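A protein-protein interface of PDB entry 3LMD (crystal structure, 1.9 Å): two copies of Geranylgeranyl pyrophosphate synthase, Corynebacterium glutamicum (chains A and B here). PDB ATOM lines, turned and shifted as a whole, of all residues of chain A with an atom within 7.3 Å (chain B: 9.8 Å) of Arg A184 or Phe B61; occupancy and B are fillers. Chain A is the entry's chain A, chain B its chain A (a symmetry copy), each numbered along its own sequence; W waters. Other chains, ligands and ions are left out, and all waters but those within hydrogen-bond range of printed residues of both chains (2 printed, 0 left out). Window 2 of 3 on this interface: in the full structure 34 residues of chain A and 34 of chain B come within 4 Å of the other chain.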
ATOM      1  N   VAL A 173       2.241  -0.114  18.755  1.00  0.00           N
ATOM      2  CA  VAL A 173       2.934   1.168  18.768  1.00  0.00           C
ATOM      3  C   VAL A 173       1.954   2.253  19.258  1.00  0.00           C
ATOM      4  O   VAL A 173       2.326   3.155  20.007  1.00  0.00           O
ATOM      5  CB  VAL A 173       3.477   1.552  17.370  1.00  0.00           C
ATOM      6  CG1 VAL A 173       4.006   2.989  17.407  1.00  0.00           C
ATOM      7  CG2 VAL A 173       4.637   0.589  16.969  1.00  0.00           C
ATOM      8  N   THR A 174       0.698   2.131  18.845  1.00  0.00           N
ATOM      9  CA  THR A 174      -0.335   3.097  19.254  1.00  0.00           C
ATOM     10  C   THR A 174      -0.490   3.024  20.782  1.00  0.00           C
ATOM     11  O   THR A 174      -0.570   4.052  21.441  1.00  0.00           O
ATOM     12  CB  THR A 174      -1.679   2.847  18.533  1.00  0.00           C
ATOM     13  OG1 THR A 174      -1.486   3.026  17.126  1.00  0.00           O
ATOM     14  CG2 THR A 174      -2.812   3.798  19.032  1.00  0.00           C
ATOM     15  N   GLY A 175      -0.512   1.814  21.340  1.00  0.00           N
ATOM     16  CA  GLY A 175      -0.618   1.651  22.801  1.00  0.00           C
ATOM     17  C   GLY A 175       0.536   2.286  23.546  1.00  0.00           C
ATOM     18  O   GLY A 175       0.337   2.941  24.581  1.00  0.00           O
ATOM     19  N   GLN A 176       1.763   2.087  23.060  1.00  0.00           N
ATOM     20  CA  GLN A 176       2.933   2.740  23.681  1.00  0.00           C
ATOM     21  C   GLN A 176       2.813   4.277  23.612  1.00  0.00           C
ATOM     22  O   GLN A 176       3.116   4.986  24.573  1.00  0.00           O
ATOM     23  CB  GLN A 176       4.239   2.293  22.977  1.00  0.00           C
ATOM     24  CG  GLN A 176       4.504   0.778  23.048  1.00  0.00           C
ATOM     25  CD  GLN A 176       5.715   0.325  22.188  1.00  0.00           C
ATOM     26  OE1 GLN A 176       5.616   0.178  20.967  1.00  0.00           O
ATOM     27  NE2 GLN A 176       6.847   0.100  22.834  1.00  0.00           N
ATOM     28  N   MET A 177       2.407   4.800  22.467  1.00  0.00           N
ATOM     29  CA  MET A 177       2.246   6.274  22.312  1.00  0.00           C
ATOM     30  C   MET A 177       1.130   6.771  23.226  1.00  0.00           C
ATOM     31  O   MET A 177       1.249   7.816  23.844  1.00  0.00           O
ATOM     32  CB  MET A 177       1.904   6.646  20.844  1.00  0.00           C
ATOM     33  CG  MET A 177       1.951   8.173  20.575  1.00  0.00           C
ATOM     34  SD  MET A 177       3.661   8.867  20.616  1.00  0.00           S
ATOM     35  CE  MET A 177       4.082   8.554  18.924  1.00  0.00           C
ATOM     36  N   ARG A 178       0.042   6.011  23.300  1.00  0.00           N
ATOM     37  CA  ARG A 178      -1.089   6.369  24.172  1.00  0.00           C
ATOM     38  C   ARG A 178      -0.651   6.439  25.634  1.00  0.00           C
ATOM     39  O   ARG A 178      -0.987   7.371  26.377  1.00  0.00           O
ATOM     40  CB  ARG A 178      -2.241   5.349  24.014  1.00  0.00           C
ATOM     41  CG  ARG A 178      -3.540   5.749  24.772  1.00  0.00           C
ATOM     42  CD  ARG A 178      -4.603   4.646  24.690  1.00  0.00           C
ATOM     43  NE  ARG A 178      -5.025   4.302  23.326  1.00  0.00           N
ATOM     44  CZ  ARG A 178      -6.013   4.927  22.678  1.00  0.00           C
ATOM     45  NH1 ARG A 178      -6.637   5.970  23.241  1.00  0.00           N
ATOM     46  NH2 ARG A 178      -6.348   4.550  21.458  1.00  0.00           N
ATOM     47  N   GLU A 179       0.109   5.450  26.058  1.00  0.00           N
ATOM     48  CA  GLU A 179       0.611   5.475  27.423  1.00  0.00           C
ATOM     49  C   GLU A 179       1.556   6.668  27.647  1.00  0.00           C
ATOM     50  O   GLU A 179       1.521   7.309  28.707  1.00  0.00           O
ATOM     51  CB  GLU A 179       1.342   4.174  27.738  1.00  0.00           C
ATOM     52  CG  GLU A 179       1.890   4.121  29.167  1.00  0.00           C
ATOM     53  CD  GLU A 179       2.631   2.833  29.418  1.00  0.00           C
ATOM     54  OE1 GLU A 179       3.410   2.419  28.531  1.00  0.00           O
ATOM     55  OE2 GLU A 179       2.419   2.227  30.487  1.00  0.00           O
ATOM     56  N   VAL A 181       1.626   9.693  25.975  1.00  0.00           N
ATOM     57  CA  VAL A 181       0.912  10.986  26.042  1.00  0.00           C
ATOM     58  C   VAL A 181      -0.048  11.102  27.229  1.00  0.00           C
ATOM     59  O   VAL A 181      -0.381  12.206  27.661  1.00  0.00           O
ATOM     60  CB  VAL A 181       0.123  11.313  24.744  1.00  0.00           C
ATOM     61  CG1 VAL A 181       1.048  11.239  23.512  1.00  0.00           C
ATOM     62  CG2 VAL A 181      -1.060  10.392  24.600  1.00  0.00           C
ATOM     63  N   GLY A 182      -0.527   9.975  27.748  1.00  0.00           N
ATOM     64  CA  GLY A 182      -1.415  10.043  28.894  1.00  0.00           C
ATOM     65  C   GLY A 182      -2.877  10.187  28.567  1.00  0.00           C
ATOM     66  O   GLY A 182      -3.269  10.263  27.400  1.00  0.00           O
ATOM     67  N   PRO A 183      -3.719  10.201  29.608  1.00  0.00           N
ATOM     68  CA  PRO A 183      -5.159  10.233  29.406  1.00  0.00           C
ATOM     69  C   PRO A 183      -5.681  11.567  28.892  1.00  0.00           C
ATOM     70  O   PRO A 183      -6.799  11.625  28.392  1.00  0.00           O
ATOM     71  CB  PRO A 183      -5.725   9.923  30.805  1.00  0.00           C
ATOM     72  CG  PRO A 183      -4.666  10.355  31.750  1.00  0.00           C
ATOM     73  CD  PRO A 183      -3.340  10.181  31.033  1.00  0.00           C
ATOM     74  N   ARG A 184      -4.877  12.623  28.992  1.00  0.00           N
ATOM     75  CA  ARG A 184      -5.331  13.961  28.585  1.00  0.00           C
ATOM     76  C   ARG A 184      -6.683  14.245  29.232  1.00  0.00           C
ATOM     77  O   ARG A 184      -6.791  14.262  30.453  1.00  0.00           O
ATOM     78  CB  ARG A 184      -5.453  14.066  27.062  1.00  0.00           C
ATOM     79  CG  ARG A 184      -4.118  13.981  26.302  1.00  0.00           C
ATOM     80  CD  ARG A 184      -4.282  13.088  25.064  1.00  0.00           C
ATOM     81  NE  ARG A 184      -4.423  11.686  25.461  1.00  0.00           N
ATOM     82  CZ  ARG A 184      -5.219  10.804  24.864  1.00  0.00           C
ATOM     83  NH1 ARG A 184      -5.974  11.171  23.835  1.00  0.00           N
ATOM     84  NH2 ARG A 184      -5.274   9.556  25.311  1.00  0.00           N
ATOM     85  N   ASP A 185      -7.710  14.431  28.409  1.00  0.00           N
ATOM     86  CA  ASP A 185      -9.048  14.749  28.900  1.00  0.00           C
ATOM     87  C   ASP A 185     -10.015  13.564  28.838  1.00  0.00           C
ATOM     88  O   ASP A 185     -11.217  13.743  29.019  1.00  0.00           O
ATOM     89  CB  ASP A 185      -9.649  15.898  28.084  1.00  0.00           C
ATOM     90  CG  ASP A 185      -9.950  15.491  26.639  1.00  0.00           C
ATOM     91  OD1 ASP A 185      -9.175  14.687  26.076  1.00  0.00           O
ATOM     92  OD2 ASP A 185     -10.959  15.966  26.063  1.00  0.00           O
ATOM     93  N   THR A 186      -9.523  12.359  28.576  1.00  0.00           N
ATOM     94  CA  THR A 186     -10.447  11.228  28.455  1.00  0.00           C
ATOM     95  C   THR A 186     -10.726  10.584  29.807  1.00  0.00           C
ATOM     96  O   THR A 186     -10.033  10.843  30.807  1.00  0.00           O
ATOM     97  CB  THR A 186      -9.901  10.147  27.512  1.00  0.00           C
ATOM     98  OG1 THR A 186      -8.670   9.638  28.042  1.00  0.00           O
ATOM     99  CG2 THR A 186      -9.659  10.728  26.129  1.00  0.00           C
ATOM    100  N   ASP A 187     -11.754   9.751  29.835  1.00  0.00           N
ATOM    101  CA  ASP A 187     -12.042   8.969  31.020  1.00  0.00           C
ATOM    102  C   ASP A 187     -10.821   8.092  31.354  1.00  0.00           C
ATOM    103  O   ASP A 187     -10.346   7.322  30.510  1.00  0.00           O
ATOM    104  CB  ASP A 187     -13.274   8.109  30.796  1.00  0.00           C
ATOM    105  CG  ASP A 187     -13.695   7.369  32.052  1.00  0.00           C
ATOM    106  OD1 ASP A 187     -12.857   6.631  32.607  1.00  0.00           O
ATOM    107  OD2 ASP A 187     -14.857   7.521  32.487  1.00  0.00           O
ATOM    108  N   PRO A 188     -10.290   8.231  32.573  1.00  0.00           N
ATOM    109  CA  PRO A 188      -9.055   7.522  32.960  1.00  0.00           C
ATOM    110  C   PRO A 188      -9.168   5.979  32.900  1.00  0.00           C
ATOM    111  O   PRO A 188      -8.170   5.295  32.677  1.00  0.00           O
ATOM    112  CB  PRO A 188      -8.814   7.988  34.408  1.00  0.00           C
ATOM    113  CG  PRO A 188      -9.732   9.218  34.610  1.00  0.00           C
ATOM    114  CD  PRO A 188     -10.842   9.088  33.653  1.00  0.00           C
ATOM    115  N   HIS A 191      -8.985   5.062  29.207  1.00  0.00           N
ATOM    116  CA  HIS A 191      -7.575   5.196  28.849  1.00  0.00           C
ATOM    117  C   HIS A 191      -6.785   3.957  29.262  1.00  0.00           C
ATOM    118  O   HIS A 191      -6.041   3.382  28.470  1.00  0.00           O
ATOM    119  CB  HIS A 191      -6.966   6.436  29.528  1.00  0.00           C
ATOM    120  CG  HIS A 191      -5.488   6.575  29.330  1.00  0.00           C
ATOM    121  ND1 HIS A 191      -4.929   6.938  28.121  1.00  0.00           N
ATOM    122  CD2 HIS A 191      -4.452   6.391  30.184  1.00  0.00           C
ATOM    123  CE1 HIS A 191      -3.615   6.991  28.246  1.00  0.00           C
ATOM    124  NE2 HIS A 191      -3.300   6.674  29.493  1.00  0.00           N
ATOM    125  N   ASN A 194      -7.746   0.969  27.132  1.00  0.00           N
ATOM    126  CA  ASN A 194      -7.202   1.086  25.765  1.00  0.00           C
ATOM    127  C   ASN A 194      -5.716   0.811  25.726  1.00  0.00           C
ATOM    128  O   ASN A 194      -5.231   0.133  24.833  1.00  0.00           O
ATOM    129  CB  ASN A 194      -7.453   2.488  25.193  1.00  0.00           C
ATOM    130  CG  ASN A 194      -8.906   2.728  24.854  1.00  0.00           C
ATOM    131  OD1 ASN A 194      -9.633   1.804  24.564  1.00  0.00           O
ATOM    132  ND2 ASN A 194      -9.328   3.972  24.899  1.00  0.00           N
ATOM    133  N   VAL A 195      -4.977   1.361  26.692  1.00  0.00           N
ATOM    134  CA  VAL A 195      -3.557   1.072  26.773  1.00  0.00           C
ATOM    135  C   VAL A 195      -3.261  -0.430  26.869  1.00  0.00           C
ATOM    136  O   VAL A 195      -2.423  -0.933  26.116  1.00  0.00           O
ATOM    137  CB  VAL A 195      -2.868   1.828  27.908  1.00  0.00           C
ATOM    138  CG1 VAL A 195      -1.424   1.309  28.065  1.00  0.00           C
ATOM    139  CG2 VAL A 195      -2.868   3.352  27.599  1.00  0.00           C
ATOM    140  N   GLU A 198      -4.139  -2.411  23.621  1.00  0.00           N
ATOM    141  CA  GLU A 198      -3.164  -2.152  22.544  1.00  0.00           C
ATOM    142  C   GLU A 198      -1.749  -2.634  22.828  1.00  0.00           C
ATOM    143  O   GLU A 198      -1.123  -3.278  21.986  1.00  0.00           O
ATOM    144  CB  GLU A 198      -3.128  -0.659  22.187  1.00  0.00           C
ATOM    145  CG  GLU A 198      -4.466  -0.191  21.610  1.00  0.00           C
ATOM    146  CD  GLU A 198      -4.598   1.325  21.619  1.00  0.00           C
ATOM    147  OE1 GLU A 198      -3.827   1.988  22.330  1.00  0.00           O
ATOM    148  OE2 GLU A 198      -5.502   1.844  20.943  1.00  0.00           O
ATOM    149  N   LEU B  55       1.095   8.867   6.509  1.00  0.00           N
ATOM    150  CA  LEU B  55       1.665   9.593   7.635  1.00  0.00           C
ATOM    151  C   LEU B  55       0.564  10.137   8.555  1.00  0.00           C
ATOM    152  O   LEU B  55       0.759  10.294   9.773  1.00  0.00           O
ATOM    153  CB  LEU B  55       2.558  10.746   7.133  1.00  0.00           C
ATOM    154  CG  LEU B  55       3.760  10.335   6.268  1.00  0.00           C
ATOM    155  CD1 LEU B  55       4.517  11.581   5.806  1.00  0.00           C
ATOM    156  CD2 LEU B  55       4.676   9.439   7.100  1.00  0.00           C
ATOM    157  N   SER B  56      -0.607  10.420   7.983  1.00  0.00           N
ATOM    158  CA  SER B  56      -1.698  10.984   8.800  1.00  0.00           C
ATOM    159  C   SER B  56      -2.757   9.943   9.149  1.00  0.00           C
ATOM    160  O   SER B  56      -3.918  10.300   9.435  1.00  0.00           O
ATOM    161  CB  SER B  56      -2.349  12.196   8.084  1.00  0.00           C
ATOM    162  OG  SER B  56      -2.832  11.817   6.794  1.00  0.00           O
ATOM    163  N   SER B  57      -2.369   8.663   9.138  1.00  0.00           N
ATOM    164  CA  SER B  57      -3.280   7.587   9.554  1.00  0.00           C
ATOM    165  C   SER B  57      -3.048   7.157  11.014  1.00  0.00           C
ATOM    166  O   SER B  57      -1.900   7.073  11.472  1.00  0.00           O
ATOM    167  CB  SER B  57      -3.115   6.364   8.638  1.00  0.00           C
ATOM    168  OG  SER B  57      -3.513   6.666   7.320  1.00  0.00           O
ATOM    169  N   GLY B  58      -4.135   6.872  11.728  1.00  0.00           N
ATOM    170  CA  GLY B  58      -4.012   6.403  13.113  1.00  0.00           C
ATOM    171  C   GLY B  58      -4.692   7.344  14.073  1.00  0.00           C
ATOM    172  O   GLY B  58      -5.364   8.319  13.652  1.00  0.00           O
ATOM    173  N   GLU B  59      -4.509   7.082  15.365  1.00  0.00           N
ATOM    174  CA  GLU B  59      -5.194   7.875  16.399  1.00  0.00           C
ATOM    175  C   GLU B  59      -4.700   9.319  16.374  1.00  0.00           C
ATOM    176  O   GLU B  59      -3.523   9.581  16.132  1.00  0.00           O
ATOM    177  CB  GLU B  59      -4.946   7.268  17.791  1.00  0.00           C
ATOM    178  CG  GLU B  59      -5.550   5.870  17.939  1.00  0.00           C
ATOM    179  CD  GLU B  59      -7.053   5.927  18.159  1.00  0.00           C
ATOM    180  OE1 GLU B  59      -7.583   7.020  18.442  1.00  0.00           O
ATOM    181  OE2 GLU B  59      -7.711   4.886  18.023  1.00  0.00           O
ATOM    182  N   ASP B  60      -5.604  10.256  16.633  1.00  0.00           N
ATOM    183  CA  ASP B  60      -5.232  11.677  16.596  1.00  0.00           C
ATOM    184  C   ASP B  60      -3.980  12.023  17.359  1.00  0.00           C
ATOM    185  O   ASP B  60      -3.116  12.753  16.851  1.00  0.00           O
ATOM    186  CB  ASP B  60      -6.396  12.598  17.020  1.00  0.00           C
ATOM    187  CG  ASP B  60      -6.982  12.282  18.416  1.00  0.00           C
ATOM    188  OD1 ASP B  60      -6.606  11.305  19.108  1.00  0.00           O
ATOM    189  OD2 ASP B  60      -7.884  13.050  18.822  1.00  0.00           O
ATOM    190  N   PHE B  61      -3.849  11.501  18.579  1.00  0.00           N
ATOM    191  CA  PHE B  61      -2.713  11.890  19.428  1.00  0.00           C
ATOM    192  C   PHE B  61      -1.400  11.403  18.840  1.00  0.00           C
ATOM    193  O   PHE B  61      -0.351  12.012  19.028  1.00  0.00           O
ATOM    194  CB  PHE B  61      -2.900  11.366  20.887  1.00  0.00           C
ATOM    195  CG  PHE B  61      -3.087   9.858  20.972  1.00  0.00           C
ATOM    196  CD1 PHE B  61      -1.989   8.995  20.891  1.00  0.00           C
ATOM    197  CD2 PHE B  61      -4.354   9.314  21.128  1.00  0.00           C
ATOM    198  CE1 PHE B  61      -2.170   7.605  20.938  1.00  0.00           C
ATOM    199  CE2 PHE B  61      -4.543   7.926  21.171  1.00  0.00           C
ATOM    200  CZ  PHE B  61      -3.438   7.074  21.083  1.00  0.00           C
ATOM    201  N   LEU B  62      -1.453  10.292  18.112  1.00  0.00           N
ATOM    202  CA  LEU B  62      -0.291   9.792  17.402  1.00  0.00           C
ATOM    203  C   LEU B  62      -0.043  10.561  16.099  1.00  0.00           C
ATOM    204  O   LEU B  62       1.097  10.974  15.788  1.00  0.00           O
ATOM    205  CB  LEU B  62      -0.467   8.289  17.119  1.00  0.00           C
ATOM    206  CG  LEU B  62       0.678   7.636  16.355  1.00  0.00           C
ATOM    207  CD1 LEU B  62       0.831   6.169  16.711  1.00  0.00           C
ATOM    208  CD2 LEU B  62       0.371   7.762  14.866  1.00  0.00           C
ATOM    209  N   VAL B  63      -1.105  10.773  15.330  1.00  0.00           N
ATOM    210  CA  VAL B  63      -0.924  11.534  14.083  1.00  0.00           C
ATOM    211  C   VAL B  63      -0.386  12.960  14.349  1.00  0.00           C
ATOM    212  O   VAL B  63       0.472  13.449  13.621  1.00  0.00           O
ATOM    213  CB  VAL B  63      -2.229  11.591  13.309  1.00  0.00           C
ATOM    214  CG1 VAL B  63      -2.121  12.570  12.162  1.00  0.00           C
ATOM    215  CG2 VAL B  63      -2.565  10.172  12.811  1.00  0.00           C
ATOM    216  N   ASP B  64      -0.870  13.608  15.401  1.00  0.00           N
ATOM    217  CA  ASP B  64      -0.357  14.967  15.731  1.00  0.00           C
ATOM    218  C   ASP B  64       1.141  14.933  15.870  1.00  0.00           C
ATOM    219  O   ASP B  64       1.850  15.821  15.397  1.00  0.00           O
ATOM    220  CB  ASP B  64      -0.959  15.491  17.028  1.00  0.00           C
ATOM    221  CG  ASP B  64      -2.409  15.834  16.877  1.00  0.00           C
ATOM    222  OD1 ASP B  64      -2.835  15.974  15.720  1.00  0.00           O
ATOM    223  OD2 ASP B  64      -3.119  15.953  17.894  1.00  0.00           O
ATOM    224  N   ILE B  65       1.641  13.890  16.525  1.00  0.00           N
ATOM    225  CA  ILE B  65       3.079  13.783  16.687  1.00  0.00           C
ATOM    226  C   ILE B  65       3.806  13.557  15.372  1.00  0.00           C
ATOM    227  O   ILE B  65       4.810  14.221  15.061  1.00  0.00           O
ATOM    228  CB  ILE B  65       3.439  12.731  17.779  1.00  0.00           C
ATOM    229  CG1 ILE B  65       3.183  13.349  19.155  1.00  0.00           C
ATOM    230  CG2 ILE B  65       4.874  12.312  17.647  1.00  0.00           C
ATOM    231  CD1 ILE B  65       2.667  12.384  20.202  1.00  0.00           C
ATOM    232  N   VAL B  66       3.298  12.639  14.555  1.00  0.00           N
ATOM    233  CA  VAL B  66       3.956  12.365  13.301  1.00  0.00           C
ATOM    234  C   VAL B  66       3.947  13.605  12.372  1.00  0.00           C
ATOM    235  O   VAL B  66       4.938  13.899  11.682  1.00  0.00           O
ATOM    236  CB  VAL B  66       3.287  11.161  12.568  1.00  0.00           C
ATOM    237  CG1 VAL B  66       3.830  11.065  11.149  1.00  0.00           C
ATOM    238  CG2 VAL B  66       3.536   9.829  13.349  1.00  0.00           C
ATOM    239  N   MET B  67       2.842  14.343  12.369  1.00  0.00           N
ATOM    240  CA  MET B  67       2.746  15.530  11.503  1.00  0.00           C
ATOM    241  C   MET B  67       3.696  16.643  11.987  1.00  0.00           C
ATOM    242  O   MET B  67       4.242  17.407  11.183  1.00  0.00           O
ATOM    243  CB  MET B  67       1.312  16.063  11.456  1.00  0.00           C
ATOM    244  CG  MET B  67       0.304  15.171  10.715  1.00  0.00           C
ATOM    245  SD  MET B  67       0.454  15.161   8.899  1.00  0.00           S
ATOM    246  CE  MET B  67       1.488  13.859   8.742  1.00  0.00           C
ATOM    247  N   HIS B  68       3.888  16.733  13.285  1.00  0.00           N
ATOM    248  CA  HIS B  68       4.811  17.701  13.805  1.00  0.00           C
ATOM    249  C   HIS B  68       6.255  17.426  13.484  1.00  0.00           C
ATOM    250  O   HIS B  68       7.047  18.329  13.438  1.00  0.00           O
ATOM    251  CB  HIS B  68       4.623  17.945  15.286  1.00  0.00           C
ATOM    252  CG  HIS B  68       5.478  19.054  15.812  1.00  0.00           C
ATOM    253  ND1 HIS B  68       5.519  20.299  15.225  1.00  0.00           N
ATOM    254  CD2 HIS B  68       6.350  19.102  16.845  1.00  0.00           C
ATOM    255  CE1 HIS B  68       6.367  21.069  15.878  1.00  0.00           C
ATOM    256  NE2 HIS B  68       6.885  20.366  16.866  1.00  0.00           N
ATOM    257  N   TRP B 134      11.088  13.175  26.422  1.00  0.00           N
ATOM    258  CA  TRP B 134       9.832  13.016  25.693  1.00  0.00           C
ATOM    259  C   TRP B 134      10.039  12.973  24.178  1.00  0.00           C
ATOM    260  O   TRP B 134       9.494  12.099  23.498  1.00  0.00           O
ATOM    261  CB  TRP B 134       8.853  14.137  26.053  1.00  0.00           C
ATOM    262  CG  TRP B 134       7.417  13.814  25.735  1.00  0.00           C
ATOM    263  CD1 TRP B 134       6.571  12.994  26.450  1.00  0.00           C
ATOM    264  CD2 TRP B 134       6.655  14.305  24.625  1.00  0.00           C
ATOM    265  NE1 TRP B 134       5.333  12.957  25.845  1.00  0.00           N
ATOM    266  CE2 TRP B 134       5.359  13.749  24.727  1.00  0.00           C
ATOM    267  CE3 TRP B 134       6.944  15.156  23.554  1.00  0.00           C
ATOM    268  CZ2 TRP B 134       4.357  14.022  23.799  1.00  0.00           C
ATOM    269  CZ3 TRP B 134       5.949  15.424  22.637  1.00  0.00           C
ATOM    270  CH2 TRP B 134       4.672  14.861  22.763  1.00  0.00           C
ATOM    271  N   VAL B 138       9.074   9.967  21.604  1.00  0.00           N
ATOM    272  CA  VAL B 138       8.070  10.065  20.564  1.00  0.00           C
ATOM    273  C   VAL B 138       8.670   9.853  19.185  1.00  0.00           C
ATOM    274  O   VAL B 138       8.011   9.291  18.321  1.00  0.00           O
ATOM    275  CB  VAL B 138       7.131  11.304  20.659  1.00  0.00           C
ATOM    276  CG1 VAL B 138       6.559  11.434  22.067  1.00  0.00           C
ATOM    277  CG2 VAL B 138       7.813  12.589  20.154  1.00  0.00           C
ATOM    278  N   LEU B 141       8.821   6.179  18.545  1.00  0.00           N
ATOM    279  CA  LEU B 141       7.502   5.657  18.238  1.00  0.00           C
ATOM    280  C   LEU B 141       6.999   6.143  16.875  1.00  0.00           C
ATOM    281  O   LEU B 141       6.300   5.402  16.167  1.00  0.00           O
ATOM    282  CB  LEU B 141       6.487   5.980  19.344  1.00  0.00           C
ATOM    283  CG  LEU B 141       6.812   5.285  20.686  1.00  0.00           C
ATOM    284  CD1 LEU B 141       5.767   5.673  21.740  1.00  0.00           C
ATOM    285  CD2 LEU B 141       6.875   3.784  20.527  1.00  0.00           C
ATOM    286  N   ALA B 142       7.329   7.369  16.500  1.00  0.00           N
ATOM    287  CA  ALA B 142       6.971   7.821  15.148  1.00  0.00           C
ATOM    288  C   ALA B 142       7.657   6.932  14.082  1.00  0.00           C
ATOM    289  O   ALA B 142       7.049   6.551  13.069  1.00  0.00           O
ATOM    290  CB  ALA B 142       7.367   9.289  14.956  1.00  0.00           C
ATOM    291  N   ILE B 145       5.711   3.545  13.995  1.00  0.00           N
ATOM    292  CA  ILE B 145       4.396   3.500  13.384  1.00  0.00           C
ATOM    293  C   ILE B 145       4.580   3.650  11.865  1.00  0.00           C
ATOM    294  O   ILE B 145       3.812   3.058  11.088  1.00  0.00           O
ATOM    295  CB  ILE B 145       3.382   4.575  13.941  1.00  0.00           C
ATOM    296  CG1 ILE B 145       1.961   4.264  13.462  1.00  0.00           C
ATOM    297  CG2 ILE B 145       3.777   6.037  13.528  1.00  0.00           C
ATOM    298  CD1 ILE B 145       1.279   3.103  14.209  1.00  0.00           C
HETATM  299  O   HOH W   1      -3.043   4.514  15.562  1.00  0.00           O
HETATM  300  O   HOH W   2      -9.156   5.819  20.926  1.00  0.00           O
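The guanidinium group (NH2) of Arg A178 lies within salt-bridge range of the side-chain carboxylate (OE2) of Glu B59, at 3.7 Å.
The guanidinium group (NE) of Arg A178 is in salt-bridge range of the side-chain carboxylate (OE1) of Glu A198 (2.8 Å). The backbone carbonyl oxygen (O) of Gly A182 lies within hydrogen-bond range of the guanidinium group (NE) of Arg A184.
CG1 of Val A173 touches O of Leu B141 (3.6 Å). Ile B145 touches Val A173 (N to CG1, 3.9 Å). Thr A174 touches Glu B59 (CG2 to CG, 3.6 Å). Thr A174 touches Phe B61. Thr A174 touches Leu B62 (OG1 to CD1, 3.9 Å). Gln A176 touches Leu B141. SD of Met A177 touches CD1 of Ile B65, at 3.7 Å. Leu B141 touches Met A177. CE2 of Phe B61 touches NH1 of Arg A178, at 3.5 Å. CG1 of Val A181 touches CD1 of Ile B65, at 3.9 Å.
Of the printed residues of chain B, Gln A176 touches Leu B141. Met A177 touches just these residues of chain B: Ile B65 (3.7 Å) and Leu B141 (3.5 Å). Glu A179 touches none of the printed residues of chain B. No residue of chain B comes within 4 Å of Asp A185. Thr A186 touches none of the printed residues of chain B. Of the printed residues of chain A, Leu B62 touches Thr A174. The nearest residue of chain A that does not touch Phe B61 is Met A177 (4.04 Å). The nearest printed residue of chain B that does not touch Thr A174 is Ile B145 (4.02 Å).
Hydrophobic or aromatic side chains of chain A that line the printed part of chain B: Val A173, Met A177 and Val A181. Printed residues of chain B that touch a printed residue of chain A: Glu B59, Phe B61, Leu B62, Ile B65, Leu B141 and Ile B145. Hydrophobic or aromatic side chains of chain B that line the printed part of chain A: Phe B61, Leu B62, Ile B65, Leu B141 and Ile B145.
No position is printed for both chains. Of the 12 pairs that touch across the chains among the printed residues, none has its exchanged pair printed and touching as well.
Water W1 bridges OG1 of Thr A174 (2.7 Å) and N of Glu B59 (3.0 Å). Water W2 bridges the guanidinium group of Arg A178 and the side-chain carboxylate of Glu B59.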
